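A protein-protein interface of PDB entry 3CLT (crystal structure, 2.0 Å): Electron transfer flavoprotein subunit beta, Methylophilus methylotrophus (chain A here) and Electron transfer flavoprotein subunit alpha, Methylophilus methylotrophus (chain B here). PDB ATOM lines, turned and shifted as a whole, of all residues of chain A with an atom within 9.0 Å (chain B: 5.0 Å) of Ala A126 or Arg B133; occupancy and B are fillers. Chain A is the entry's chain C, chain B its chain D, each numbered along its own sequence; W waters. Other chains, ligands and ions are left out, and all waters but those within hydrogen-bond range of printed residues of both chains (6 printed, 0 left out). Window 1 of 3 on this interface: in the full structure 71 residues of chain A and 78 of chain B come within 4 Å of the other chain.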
ATOM      1  N   LYS A   8      31.838  -0.829 -14.813  1.00  0.00           N
ATOM      2  CA  LYS A   8      30.880   0.265 -14.721  1.00  0.00           C
ATOM      3  C   LYS A   8      29.456  -0.287 -14.654  1.00  0.00           C
ATOM      4  O   LYS A   8      29.084  -1.180 -15.432  1.00  0.00           O
ATOM      5  CB  LYS A   8      30.995   1.188 -15.937  1.00  0.00           C
ATOM      6  CG  LYS A   8      30.145   2.465 -15.843  1.00  0.00           C
ATOM      7  CD  LYS A   8      30.209   3.320 -17.093  1.00  0.00           C
ATOM      8  CE  LYS A   8      29.354   4.580 -16.928  1.00  0.00           C
ATOM      9  NZ  LYS A   8      29.375   5.484 -18.129  1.00  0.00           N
ATOM     10  N   THR A  10      26.104   0.828 -15.710  1.00  0.00           N
ATOM     11  CA  THR A  10      25.565   1.752 -16.685  1.00  0.00           C
ATOM     12  C   THR A  10      24.080   2.005 -16.432  1.00  0.00           C
ATOM     13  O   THR A  10      23.414   1.241 -15.722  1.00  0.00           O
ATOM     14  CB  THR A  10      25.757   1.206 -18.119  1.00  0.00           C
ATOM     15  OG1 THR A  10      25.379  -0.173 -18.164  1.00  0.00           O
ATOM     16  CG2 THR A  10      27.196   1.339 -18.563  1.00  0.00           C
ATOM     17  N   ALA A  11      23.583   3.090 -17.023  1.00  0.00           N
ATOM     18  CA  ALA A  11      22.184   3.483 -16.950  1.00  0.00           C
ATOM     19  C   ALA A  11      21.542   3.341 -18.320  1.00  0.00           C
ATOM     20  O   ALA A  11      22.135   3.713 -19.342  1.00  0.00           O
ATOM     21  CB  ALA A  11      22.076   4.917 -16.484  1.00  0.00           C
ATOM     22  N   ASN A  36      27.569  -2.959 -17.071  1.00  0.00           N
ATOM     23  CA  ASN A  36      27.921  -2.777 -18.483  1.00  0.00           C
ATOM     24  C   ASN A  36      28.159  -4.129 -19.176  1.00  0.00           C
ATOM     25  O   ASN A  36      28.866  -4.998 -18.648  1.00  0.00           O
ATOM     26  CB  ASN A  36      29.169  -1.897 -18.585  1.00  0.00           C
ATOM     27  CG  ASN A  36      29.546  -1.567 -20.022  1.00  0.00           C
ATOM     28  OD1 ASN A  36      28.675  -1.318 -20.873  1.00  0.00           O
ATOM     29  ND2 ASN A  36      30.845  -1.565 -20.298  1.00  0.00           N
ATOM     30  N   TRP A  38      29.957  -5.113 -21.698  1.00  0.00           N
ATOM     31  CA  TRP A  38      31.378  -5.430 -21.934  1.00  0.00           C
ATOM     32  C   TRP A  38      32.079  -6.005 -20.694  1.00  0.00           C
ATOM     33  O   TRP A  38      32.988  -6.846 -20.807  1.00  0.00           O
ATOM     34  CB  TRP A  38      32.131  -4.181 -22.443  1.00  0.00           C
ATOM     35  CG  TRP A  38      31.908  -3.937 -23.911  1.00  0.00           C
ATOM     36  CD1 TRP A  38      32.730  -4.316 -24.937  1.00  0.00           C
ATOM     37  CD2 TRP A  38      30.781  -3.296 -24.519  1.00  0.00           C
ATOM     38  NE1 TRP A  38      32.186  -3.945 -26.143  1.00  0.00           N
ATOM     39  CE2 TRP A  38      30.989  -3.325 -25.920  1.00  0.00           C
ATOM     40  CE3 TRP A  38      29.616  -2.688 -24.020  1.00  0.00           C
ATOM     41  CZ2 TRP A  38      30.079  -2.783 -26.823  1.00  0.00           C
ATOM     42  CZ3 TRP A  38      28.708  -2.157 -24.926  1.00  0.00           C
ATOM     43  CH2 TRP A  38      28.946  -2.211 -26.309  1.00  0.00           C
ATOM     44  N   ASP A  96      34.617  12.779 -16.102  1.00  0.00           N
ATOM     45  CA  ASP A  96      34.605  12.143 -17.428  1.00  0.00           C
ATOM     46  C   ASP A  96      35.520  10.903 -17.448  1.00  0.00           C
ATOM     47  O   ASP A  96      36.025  10.487 -16.403  1.00  0.00           O
ATOM     48  CB  ASP A  96      34.942  13.171 -18.524  1.00  0.00           C
ATOM     49  CG  ASP A  96      36.416  13.558 -18.571  1.00  0.00           C
ATOM     50  OD1 ASP A  96      37.204  13.119 -17.703  1.00  0.00           O
ATOM     51  OD2 ASP A  96      36.773  14.332 -19.493  1.00  0.00           O
ATOM     52  N   ALA A  97      35.725  10.320 -18.633  1.00  0.00           N
ATOM     53  CA  ALA A  97      36.517   9.091 -18.779  1.00  0.00           C
ATOM     54  C   ALA A  97      37.950   9.259 -18.276  1.00  0.00           C
ATOM     55  O   ALA A  97      38.540   8.325 -17.733  1.00  0.00           O
ATOM     56  CB  ALA A  97      36.547   8.656 -20.233  1.00  0.00           C
ATOM     57  N   VAL A 120      35.666  -2.411 -23.789  1.00  0.00           N
ATOM     58  CA  VAL A 120      35.923  -1.532 -24.935  1.00  0.00           C
ATOM     59  C   VAL A 120      35.224  -0.190 -24.775  1.00  0.00           C
ATOM     60  O   VAL A 120      35.842   0.856 -24.994  1.00  0.00           O
ATOM     61  CB  VAL A 120      35.513  -2.195 -26.282  1.00  0.00           C
ATOM     62  CG1 VAL A 120      35.393  -1.168 -27.412  1.00  0.00           C
ATOM     63  CG2 VAL A 120      36.511  -3.261 -26.649  1.00  0.00           C
ATOM     64  N   GLN A 121      33.938  -0.228 -24.416  1.00  0.00           N
ATOM     65  CA  GLN A 121      33.147   0.972 -24.177  1.00  0.00           C
ATOM     66  C   GLN A 121      31.981   0.680 -23.221  1.00  0.00           C
ATOM     67  O   GLN A 121      31.720  -0.474 -22.889  1.00  0.00           O
ATOM     68  CB  GLN A 121      32.612   1.533 -25.489  1.00  0.00           C
ATOM     69  CG  GLN A 121      31.654   0.600 -26.218  1.00  0.00           C
ATOM     70  CD  GLN A 121      31.122   1.202 -27.494  1.00  0.00           C
ATOM     71  OE1 GLN A 121      29.914   1.212 -27.718  1.00  0.00           O
ATOM     72  NE2 GLN A 121      32.012   1.744 -28.316  1.00  0.00           N
ATOM     73  N   SER A 122      31.318   1.750 -22.762  1.00  0.00           N
ATOM     74  CA  SER A 122      30.120   1.646 -21.916  1.00  0.00           C
ATOM     75  C   SER A 122      28.883   1.763 -22.792  1.00  0.00           C
ATOM     76  O   SER A 122      28.873   2.505 -23.776  1.00  0.00           O
ATOM     77  CB  SER A 122      30.100   2.727 -20.824  1.00  0.00           C
ATOM     78  OG  SER A 122      30.257   4.025 -21.368  1.00  0.00           O
ATOM     79  N   SER A 123      27.842   1.016 -22.448  1.00  0.00           N
ATOM     80  CA  SER A 123      26.629   1.002 -23.258  1.00  0.00           C
ATOM     81  C   SER A 123      25.887   2.336 -23.188  1.00  0.00           C
ATOM     82  O   SER A 123      25.126   2.662 -24.099  1.00  0.00           O
ATOM     83  CB  SER A 123      25.695  -0.133 -22.826  1.00  0.00           C
ATOM     84  OG  SER A 123      25.376  -0.020 -21.455  1.00  0.00           O
ATOM     85  N   ASP A 124      26.096   3.103 -22.116  1.00  0.00           N
ATOM     86  CA  ASP A 124      25.403   4.378 -21.988  1.00  0.00           C
ATOM     87  C   ASP A 124      26.119   5.497 -22.742  1.00  0.00           C
ATOM     88  O   ASP A 124      25.596   6.028 -23.732  1.00  0.00           O
ATOM     89  CB  ASP A 124      25.059   4.755 -20.522  1.00  0.00           C
ATOM     90  CG  ASP A 124      26.220   4.600 -19.540  1.00  0.00           C
ATOM     91  OD1 ASP A 124      27.390   4.547 -19.952  1.00  0.00           O
ATOM     92  OD2 ASP A 124      25.938   4.567 -18.322  1.00  0.00           O
ATOM     93  N   GLN A 125      27.325   5.823 -22.322  1.00  0.00           N
ATOM     94  CA  GLN A 125      28.015   6.988 -22.873  1.00  0.00           C
ATOM     95  C   GLN A 125      28.935   6.627 -24.056  1.00  0.00           C
ATOM     96  O   GLN A 125      29.245   7.481 -24.901  1.00  0.00           O
ATOM     97  CB  GLN A 125      28.773   7.707 -21.745  1.00  0.00           C
ATOM     98  CG  GLN A 125      27.950   8.728 -20.866  1.00  0.00           C
ATOM     99  CD  GLN A 125      26.404   8.513 -20.744  1.00  0.00           C
ATOM    100  OE1 GLN A 125      25.665   8.531 -21.726  1.00  0.00           O
ATOM    101  NE2 GLN A 125      25.925   8.408 -19.501  1.00  0.00           N
ATOM    102  N   ALA A 126      29.376   5.371 -24.115  1.00  0.00           N
ATOM    103  CA  ALA A 126      30.175   4.883 -25.235  1.00  0.00           C
ATOM    104  C   ALA A 126      31.332   5.825 -25.574  1.00  0.00           C
ATOM    105  O   ALA A 126      31.518   6.217 -26.735  1.00  0.00           O
ATOM    106  CB  ALA A 126      29.280   4.655 -26.448  1.00  0.00           C
ATOM    107  N   TYR A 127      32.095   6.192 -24.546  1.00  0.00           N
ATOM    108  CA  TYR A 127      33.282   7.038 -24.712  1.00  0.00           C
ATOM    109  C   TYR A 127      34.401   6.261 -25.399  1.00  0.00           C
ATOM    110  O   TYR A 127      35.201   6.845 -26.150  1.00  0.00           O
ATOM    111  CB  TYR A 127      33.825   7.523 -23.359  1.00  0.00           C
ATOM    112  CG  TYR A 127      32.909   8.403 -22.541  1.00  0.00           C
ATOM    113  CD1 TYR A 127      32.629   8.091 -21.212  1.00  0.00           C
ATOM    114  CD2 TYR A 127      32.366   9.571 -23.070  1.00  0.00           C
ATOM    115  CE1 TYR A 127      31.809   8.898 -20.434  1.00  0.00           C
ATOM    116  CE2 TYR A 127      31.538  10.399 -22.301  1.00  0.00           C
ATOM    117  CZ  TYR A 127      31.256  10.052 -20.985  1.00  0.00           C
ATOM    118  OH  TYR A 127      30.431  10.838 -20.197  1.00  0.00           O
ATOM    119  N   ALA A 128      34.456   4.957 -25.123  1.00  0.00           N
ATOM    120  CA  ALA A 128      35.564   4.086 -25.530  1.00  0.00           C
ATOM    121  C   ALA A 128      36.913   4.747 -25.205  1.00  0.00           C
ATOM    122  O   ALA A 128      37.800   4.844 -26.074  1.00  0.00           O
ATOM    123  CB  ALA A 128      35.460   3.732 -27.017  1.00  0.00           C
ATOM    124  N   SER A 129      37.032   5.220 -23.959  1.00  0.00           N
ATOM    125  CA  SER A 129      38.175   6.027 -23.509  1.00  0.00           C
ATOM    126  C   SER A 129      38.759   5.643 -22.159  1.00  0.00           C
ATOM    127  O   SER A 129      39.941   5.860 -21.923  1.00  0.00           O
ATOM    128  CB  SER A 129      37.776   7.504 -23.424  1.00  0.00           C
ATOM    129  OG  SER A 129      37.502   8.035 -24.705  1.00  0.00           O
ATOM    130  N   THR A 130      37.940   5.101 -21.262  1.00  0.00           N
ATOM    131  CA  THR A 130      38.343   4.968 -19.863  1.00  0.00           C
ATOM    132  C   THR A 130      39.518   4.023 -19.624  1.00  0.00           C
ATOM    133  O   THR A 130      40.481   4.381 -18.928  1.00  0.00           O
ATOM    134  CB  THR A 130      37.136   4.572 -18.990  1.00  0.00           C
ATOM    135  OG1 THR A 130      36.095   5.548 -19.169  1.00  0.00           O
ATOM    136  CG2 THR A 130      37.520   4.545 -17.518  1.00  0.00           C
ATOM    137  N   SER A 227      36.273  18.032 -21.098  1.00  0.00           N
ATOM    138  CA  SER A 227      35.260  18.779 -21.832  1.00  0.00           C
ATOM    139  C   SER A 227      34.191  19.158 -20.807  1.00  0.00           C
ATOM    140  O   SER A 227      34.085  18.519 -19.747  1.00  0.00           O
ATOM    141  CB  SER A 227      34.650  17.956 -22.969  1.00  0.00           C
ATOM    142  OG  SER A 227      33.921  16.832 -22.481  1.00  0.00           O
ATOM    143  N   VAL A 229      30.050  19.768 -20.337  1.00  0.00           N
ATOM    144  CA  VAL A 229      28.701  19.614 -20.866  1.00  0.00           C
ATOM    145  C   VAL A 229      27.997  20.964 -20.843  1.00  0.00           C
ATOM    146  O   VAL A 229      27.889  21.584 -19.795  1.00  0.00           O
ATOM    147  CB  VAL A 229      27.855  18.600 -20.055  1.00  0.00           C
ATOM    148  CG1 VAL A 229      26.429  18.515 -20.629  1.00  0.00           C
ATOM    149  CG2 VAL A 229      28.500  17.236 -20.068  1.00  0.00           C
ATOM    150  N   ARG A 231      24.844  21.230 -22.521  1.00  0.00           N
ATOM    151  CA  ARG A 231      23.488  20.737 -22.361  1.00  0.00           C
ATOM    152  C   ARG A 231      23.349  19.319 -22.892  1.00  0.00           C
ATOM    153  O   ARG A 231      24.149  18.858 -23.729  1.00  0.00           O
ATOM    154  CB  ARG A 231      22.484  21.628 -23.101  1.00  0.00           C
ATOM    155  CG  ARG A 231      22.784  21.768 -24.587  1.00  0.00           C
ATOM    156  CD  ARG A 231      21.614  22.331 -25.349  1.00  0.00           C
ATOM    157  NE  ARG A 231      21.980  22.567 -26.744  1.00  0.00           N
ATOM    158  CZ  ARG A 231      21.138  22.563 -27.774  1.00  0.00           C
ATOM    159  NH1 ARG A 231      19.840  22.338 -27.595  1.00  0.00           N
ATOM    160  NH2 ARG A 231      21.602  22.795 -29.002  1.00  0.00           N
ATOM    161  N   MET A 232      22.300  18.665 -22.421  1.00  0.00           N
ATOM    162  CA  MET A 232      21.874  17.389 -22.933  1.00  0.00           C
ATOM    163  C   MET A 232      20.436  17.608 -23.390  1.00  0.00           C
ATOM    164  O   MET A 232      19.647  18.238 -22.681  1.00  0.00           O
ATOM    165  CB  MET A 232      21.961  16.359 -21.817  1.00  0.00           C
ATOM    166  CG  MET A 232      21.912  14.935 -22.265  1.00  0.00           C
ATOM    167  SD  MET A 232      22.122  13.833 -20.858  1.00  0.00           S
ATOM    168  CE  MET A 232      23.884  13.582 -20.806  1.00  0.00           C
ATOM    169  N   TYR A 233      20.099  17.122 -24.583  1.00  0.00           N
ATOM    170  CA  TYR A 233      18.767  17.330 -25.129  1.00  0.00           C
ATOM    171  C   TYR A 233      18.361  16.146 -25.979  1.00  0.00           C
ATOM    172  O   TYR A 233      19.208  15.392 -26.457  1.00  0.00           O
ATOM    173  CB  TYR A 233      18.704  18.638 -25.930  1.00  0.00           C
ATOM    174  CG  TYR A 233      19.616  18.682 -27.137  1.00  0.00           C
ATOM    175  CD1 TYR A 233      19.134  18.376 -28.409  1.00  0.00           C
ATOM    176  CD2 TYR A 233      20.955  19.046 -27.014  1.00  0.00           C
ATOM    177  CE1 TYR A 233      19.964  18.423 -29.529  1.00  0.00           C
ATOM    178  CE2 TYR A 233      21.790  19.096 -28.128  1.00  0.00           C
ATOM    179  CZ  TYR A 233      21.283  18.785 -29.380  1.00  0.00           C
ATOM    180  OH  TYR A 233      22.102  18.847 -30.484  1.00  0.00           O
ATOM    181  N   PRO A 235      17.282  14.943 -29.268  1.00  0.00           N
ATOM    182  CA  PRO A 235      17.299  15.545 -30.597  1.00  0.00           C
ATOM    183  C   PRO A 235      16.069  15.139 -31.415  1.00  0.00           C
ATOM    184  O   PRO A 235      15.357  14.204 -31.046  1.00  0.00           O
ATOM    185  CB  PRO A 235      18.575  14.985 -31.209  1.00  0.00           C
ATOM    186  CG  PRO A 235      18.731  13.629 -30.573  1.00  0.00           C
ATOM    187  CD  PRO A 235      18.199  13.793 -29.163  1.00  0.00           C
ATOM    188  N   LYS A 237      14.973  13.120 -34.278  1.00  0.00           N
ATOM    189  CA  LYS A 237      15.598  12.039 -35.024  1.00  0.00           C
ATOM    190  C   LYS A 237      14.685  11.644 -36.172  1.00  0.00           C
ATOM    191  O   LYS A 237      13.533  12.093 -36.249  1.00  0.00           O
ATOM    192  CB  LYS A 237      15.922  10.851 -34.111  1.00  0.00           C
ATOM    193  CG  LYS A 237      16.918  11.201 -32.984  1.00  0.00           C
ATOM    194  CD  LYS A 237      17.938  10.090 -32.705  1.00  0.00           C
ATOM    195  CE  LYS A 237      18.325   9.989 -31.227  1.00  0.00           C
ATOM    196  NZ  LYS A 237      19.656  10.589 -30.901  1.00  0.00           N
ATOM    197  N   HIS B  96      37.128   7.944 -35.240  1.00  0.00           N
ATOM    198  CA  HIS B  96      36.698   7.084 -34.142  1.00  0.00           C
ATOM    199  C   HIS B  96      36.743   5.656 -34.665  1.00  0.00           C
ATOM    200  O   HIS B  96      35.738   5.050 -34.991  1.00  0.00           O
ATOM    201  CB  HIS B  96      35.312   7.455 -33.619  1.00  0.00           C
ATOM    202  CG  HIS B  96      34.985   6.831 -32.296  1.00  0.00           C
ATOM    203  ND1 HIS B  96      35.671   7.140 -31.142  1.00  0.00           N
ATOM    204  CD2 HIS B  96      34.057   5.908 -31.951  1.00  0.00           C
ATOM    205  CE1 HIS B  96      35.163   6.449 -30.137  1.00  0.00           C
ATOM    206  NE2 HIS B  96      34.179   5.697 -30.601  1.00  0.00           N
ATOM    207  N   ALA B 116      37.042  14.855 -26.661  1.00  0.00           N
ATOM    208  CA  ALA B 116      35.731  14.204 -26.766  1.00  0.00           C
ATOM    209  C   ALA B 116      35.758  13.190 -27.896  1.00  0.00           C
ATOM    210  O   ALA B 116      36.475  13.367 -28.876  1.00  0.00           O
ATOM    211  CB  ALA B 116      34.639  15.208 -27.003  1.00  0.00           C
ATOM    212  N   THR B 117      34.963  12.136 -27.770  1.00  0.00           N
ATOM    213  CA  THR B 117      35.012  11.035 -28.731  1.00  0.00           C
ATOM    214  C   THR B 117      33.691  10.779 -29.453  1.00  0.00           C
ATOM    215  O   THR B 117      32.623  11.125 -28.965  1.00  0.00           O
ATOM    216  CB  THR B 117      35.462   9.711 -28.064  1.00  0.00           C
ATOM    217  OG1 THR B 117      34.503   9.299 -27.090  1.00  0.00           O
ATOM    218  CG2 THR B 117      36.819   9.867 -27.404  1.00  0.00           C
ATOM    219  N   ASP B 118      33.796  10.165 -30.625  1.00  0.00           N
ATOM    220  CA  ASP B 118      32.640   9.739 -31.420  1.00  0.00           C
ATOM    221  C   ASP B 118      31.676  10.923 -31.681  1.00  0.00           C
ATOM    222  O   ASP B 118      30.449  10.820 -31.537  1.00  0.00           O
ATOM    223  CB  ASP B 118      31.942   8.546 -30.745  1.00  0.00           C
ATOM    224  CG  ASP B 118      30.986   7.809 -31.684  1.00  0.00           C
ATOM    225  OD1 ASP B 118      31.161   7.900 -32.926  1.00  0.00           O
ATOM    226  OD2 ASP B 118      30.067   7.130 -31.174  1.00  0.00           O
ATOM    227  N   VAL B 119      32.287  12.031 -32.089  1.00  0.00           N
ATOM    228  CA  VAL B 119      31.620  13.300 -32.314  1.00  0.00           C
ATOM    229  C   VAL B 119      30.985  13.301 -33.692  1.00  0.00           C
ATOM    230  O   VAL B 119      31.624  12.898 -34.671  1.00  0.00           O
ATOM    231  CB  VAL B 119      32.638  14.464 -32.198  1.00  0.00           C
ATOM    232  CG1 VAL B 119      32.050  15.793 -32.711  1.00  0.00           C
ATOM    233  CG2 VAL B 119      33.094  14.605 -30.755  1.00  0.00           C
ATOM    234  N   TYR B 120      29.733  13.751 -33.766  1.00  0.00           N
ATOM    235  CA  TYR B 120      29.017  13.790 -35.041  1.00  0.00           C
ATOM    236  C   TYR B 120      28.390  15.140 -35.415  1.00  0.00           C
ATOM    237  O   TYR B 120      27.736  15.248 -36.461  1.00  0.00           O
ATOM    238  CB  TYR B 120      27.988  12.659 -35.111  1.00  0.00           C
ATOM    239  CG  TYR B 120      27.045  12.540 -33.946  1.00  0.00           C
ATOM    240  CD1 TYR B 120      25.907  13.333 -33.860  1.00  0.00           C
ATOM    241  CD2 TYR B 120      27.255  11.595 -32.958  1.00  0.00           C
ATOM    242  CE1 TYR B 120      25.020  13.199 -32.795  1.00  0.00           C
ATOM    243  CE2 TYR B 120      26.369  11.455 -31.894  1.00  0.00           C
ATOM    244  CZ  TYR B 120      25.251  12.245 -31.829  1.00  0.00           C
ATOM    245  OH  TYR B 120      24.361  12.109 -30.777  1.00  0.00           O
ATOM    246  N   ALA B 131      31.194  20.749 -29.709  1.00  0.00           N
ATOM    247  CA  ALA B 131      31.118  19.406 -30.242  1.00  0.00           C
ATOM    248  C   ALA B 131      29.886  18.698 -29.689  1.00  0.00           C
ATOM    249  O   ALA B 131      29.519  18.888 -28.527  1.00  0.00           O
ATOM    250  CB  ALA B 131      32.368  18.637 -29.861  1.00  0.00           C
ATOM    251  N   THR B 132      29.271  17.855 -30.515  1.00  0.00           N
ATOM    252  CA  THR B 132      28.103  17.093 -30.078  1.00  0.00           C
ATOM    253  C   THR B 132      28.329  15.604 -30.268  1.00  0.00           C
ATOM    254  O   THR B 132      28.779  15.142 -31.318  1.00  0.00           O
ATOM    255  CB  THR B 132      26.822  17.525 -30.807  1.00  0.00           C
ATOM    256  OG1 THR B 132      26.696  18.951 -30.731  1.00  0.00           O
ATOM    257  CG2 THR B 132      25.587  16.856 -30.183  1.00  0.00           C
ATOM    258  N   ARG B 133      28.011  14.871 -29.218  1.00  0.00           N
ATOM    259  CA  ARG B 133      28.107  13.429 -29.218  1.00  0.00           C
ATOM    260  C   ARG B 133      26.816  12.874 -28.611  1.00  0.00           C
ATOM    261  O   ARG B 133      25.894  13.633 -28.280  1.00  0.00           O
ATOM    262  CB  ARG B 133      29.361  12.993 -28.440  1.00  0.00           C
ATOM    263  CG  ARG B 133      29.258  13.138 -26.923  1.00  0.00           C
ATOM    264  CD  ARG B 133      30.546  12.782 -26.193  1.00  0.00           C
ATOM    265  NE  ARG B 133      31.114  11.518 -26.651  1.00  0.00           N
ATOM    266  CZ  ARG B 133      30.686  10.314 -26.269  1.00  0.00           C
ATOM    267  NH1 ARG B 133      29.676  10.187 -25.410  1.00  0.00           N
ATOM    268  NH2 ARG B 133      31.268   9.221 -26.753  1.00  0.00           N
ATOM    269  N   GLY B 134      26.734  11.552 -28.506  1.00  0.00           N
ATOM    270  CA  GLY B 134      25.557  10.911 -27.959  1.00  0.00           C
ATOM    271  C   GLY B 134      25.626  10.685 -26.463  1.00  0.00           C
ATOM    272  O   GLY B 134      26.690  10.783 -25.838  1.00  0.00           O
ATOM    273  N   GLY B 135      24.468  10.382 -25.887  1.00  0.00           N
ATOM    274  CA  GLY B 135      24.380   9.913 -24.512  1.00  0.00           C
ATOM    275  C   GLY B 135      23.284   8.878 -24.395  1.00  0.00           C
ATOM    276  O   GLY B 135      22.332   8.853 -25.210  1.00  0.00           O
ATOM    277  N   VAL B 140      20.018  10.632 -26.373  1.00  0.00           N
ATOM    278  CA  VAL B 140      20.165  12.085 -26.319  1.00  0.00           C
ATOM    279  C   VAL B 140      21.380  12.547 -27.117  1.00  0.00           C
ATOM    280  O   VAL B 140      22.227  11.740 -27.521  1.00  0.00           O
ATOM    281  CB  VAL B 140      20.276  12.604 -24.849  1.00  0.00           C
ATOM    282  CG1 VAL B 140      19.016  12.244 -24.043  1.00  0.00           C
ATOM    283  CG2 VAL B 140      21.520  12.057 -24.165  1.00  0.00           C
ATOM    284  N   ASN B 141      21.440  13.856 -27.346  1.00  0.00           N
ATOM    285  CA  ASN B 141      22.662  14.521 -27.752  1.00  0.00           C
ATOM    286  C   ASN B 141      23.262  15.213 -26.535  1.00  0.00           C
ATOM    287  O   ASN B 141      22.537  15.772 -25.711  1.00  0.00           O
ATOM    288  CB  ASN B 141      22.387  15.548 -28.849  1.00  0.00           C
ATOM    289  CG  ASN B 141      22.233  14.917 -30.226  1.00  0.00           C
ATOM    290  OD1 ASN B 141      22.289  13.695 -30.385  1.00  0.00           O
ATOM    291  ND2 ASN B 141      22.037  15.756 -31.224  1.00  0.00           N
ATOM    292  N   VAL B 142      24.582  15.136 -26.417  1.00  0.00           N
ATOM    293  CA  VAL B 142      25.324  15.845 -25.381  1.00  0.00           C
ATOM    294  C   VAL B 142      26.223  16.845 -26.100  1.00  0.00           C
ATOM    295  O   VAL B 142      27.080  16.464 -26.902  1.00  0.00           O
ATOM    296  CB  VAL B 142      26.168  14.868 -24.524  1.00  0.00           C
ATOM    297  CG1 VAL B 142      26.847  15.592 -23.372  1.00  0.00           C
ATOM    298  CG2 VAL B 142      25.291  13.709 -24.021  1.00  0.00           C
HETATM  299  O   HOH W   1      25.293   7.220 -26.273  1.00  0.00           O
HETATM  300  O   HOH W   2      29.599   7.282 -28.616  1.00  0.00           O
HETATM  301  O   HOH W   3      24.222  20.234 -30.392  1.00  0.00           O
HETATM  302  O   HOH W   4      32.395   4.367 -28.920  1.00  0.00           O
HETATM  303  O   HOH W   5      21.263  11.958 -32.694  1.00  0.00           O
HETATM  304  O   HOH W   6      27.483   8.198 -27.287  1.00  0.00           O
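Among the printed residues, pairs that only touch across the chains: Asp A124 with Gly B135 (3.7 Å), Gln A125 with Gly B135 (3.4 Å), Tyr A127 with Arg B133 (3.6 Å), Ser A129 with Thr B117 (3.3 Å), Arg A231 with Val B142 (3.6 Å), Met A232 with Val B140 (3.5 Å), Met A232 with Asn B141 (3.3 Å), Met A232 with Val B142 (3.5 Å), Tyr A233 with Val B140 (3.4 Å), Pro A235 with Val B140 (3.9 Å) and Pro A235 with Asn B141 (3.5 Å).
Of the 14 printed residues of chain B, 6 touch a printed residue of chain A. Hydrophobic or aromatic side chains of chain B that line the printed part of chain A: Val B140 and Val B142. Along chain A the printed residues that touch a printed residue of chain B span positions 124 to 235. Among the printed residues, 15 pairs touch across the chains. Among the printed residues, no Asp or Glu carboxylate lies within 4 Å of a Lys or Arg side-chain nitrogen of the other chain.
Ser A123 touches none of the printed residues of chain B. Of the printed residues of chain B, Tyr A127 touches Thr B117 and Arg B133. Printed residues of chain B within 4 Å of Tyr A233: Val B140 and Asn B141. Of the printed residues of chain A, Thr B117 touches Tyr A127 and Ser A129. No residue of chain A comes within 4 Å of Thr B132. Arg B133 touches three residues of chain A. The nearest residue of chain B that does not touch Ala A126 is Thr B117 (4.3 Å).
The backbone NH (N) of Asn B141 lies within hydrogen-bond range of the backbone carbonyl oxygen (O) of Tyr A233 (2.9 Å). The guanidinium group of Arg B133 sits at hydrogen-bond distance from the backbone carbonyl oxygen of Gln A125 (2.8 Å). O of Ala A126 sits at hydrogen-bond distance from NH2 of Arg B133, 3.0 Å away. The backbone carbonyl oxygen (O) of Tyr A127 is in hydrogen-bond range of the side-chain hydroxyl (OG1) of Thr B117.
The backbone NH (N) of Gly B135 is in hydrogen-bond range of the backbone carbonyl oxygen (O) of Val B140 (3.1 Å). The backbone NH of Ala A11 is in hydrogen-bond range of the side-chain carboxylate of Asp A124. N of Val B142 is in hydrogen-bond range of O of Arg B133, 2.7 Å away. The side-chain carboxylate (OD1) of Asp A124 is in salt-bridge range of the side-chain amino group (NZ) of Lys A8. OH of Tyr B120 is in hydrogen-bond range of O of Arg B133. O of Tyr A127 is in hydrogen-bond range of OG of Ser A129 (3.0 Å).
Water W3 bridges the side-chain hydroxyl (OH) of Tyr A233 (2.5 Å) and the side-chain hydroxyl (OG1) of Thr B132 (2.8 Å). Water W2 lies within hydrogen-bond range of the side-chain carboxylate (OD2) of Asp B118 (2.6 Å), the backbone carbonyl oxygen (O) of Ala A126 (2.9 Å) and the guanidinium group (NH2) of Arg B133 (3.2 Å). Water W4 lies within hydrogen-bond range of the side-chain amide nitrogen of Gln A121 (2.7 Å), a ring nitrogen (NE2) of His B96 (2.8 Å) and the backbone carbonyl oxygen of Ala A126 (3.0 Å). Water W5 bridges NZ of Lys A237 (2.8 Å) and OD1 of Asn B141 (3.1 Å). Water W1 lies within hydrogen-bond range of O of Asp A124 (2.8 Å) and N of Gly B135 (3.3 Å). Water W6 bridges O of Gln A125 (3.1 Å) and O of Gly B134 (3.1 Å).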
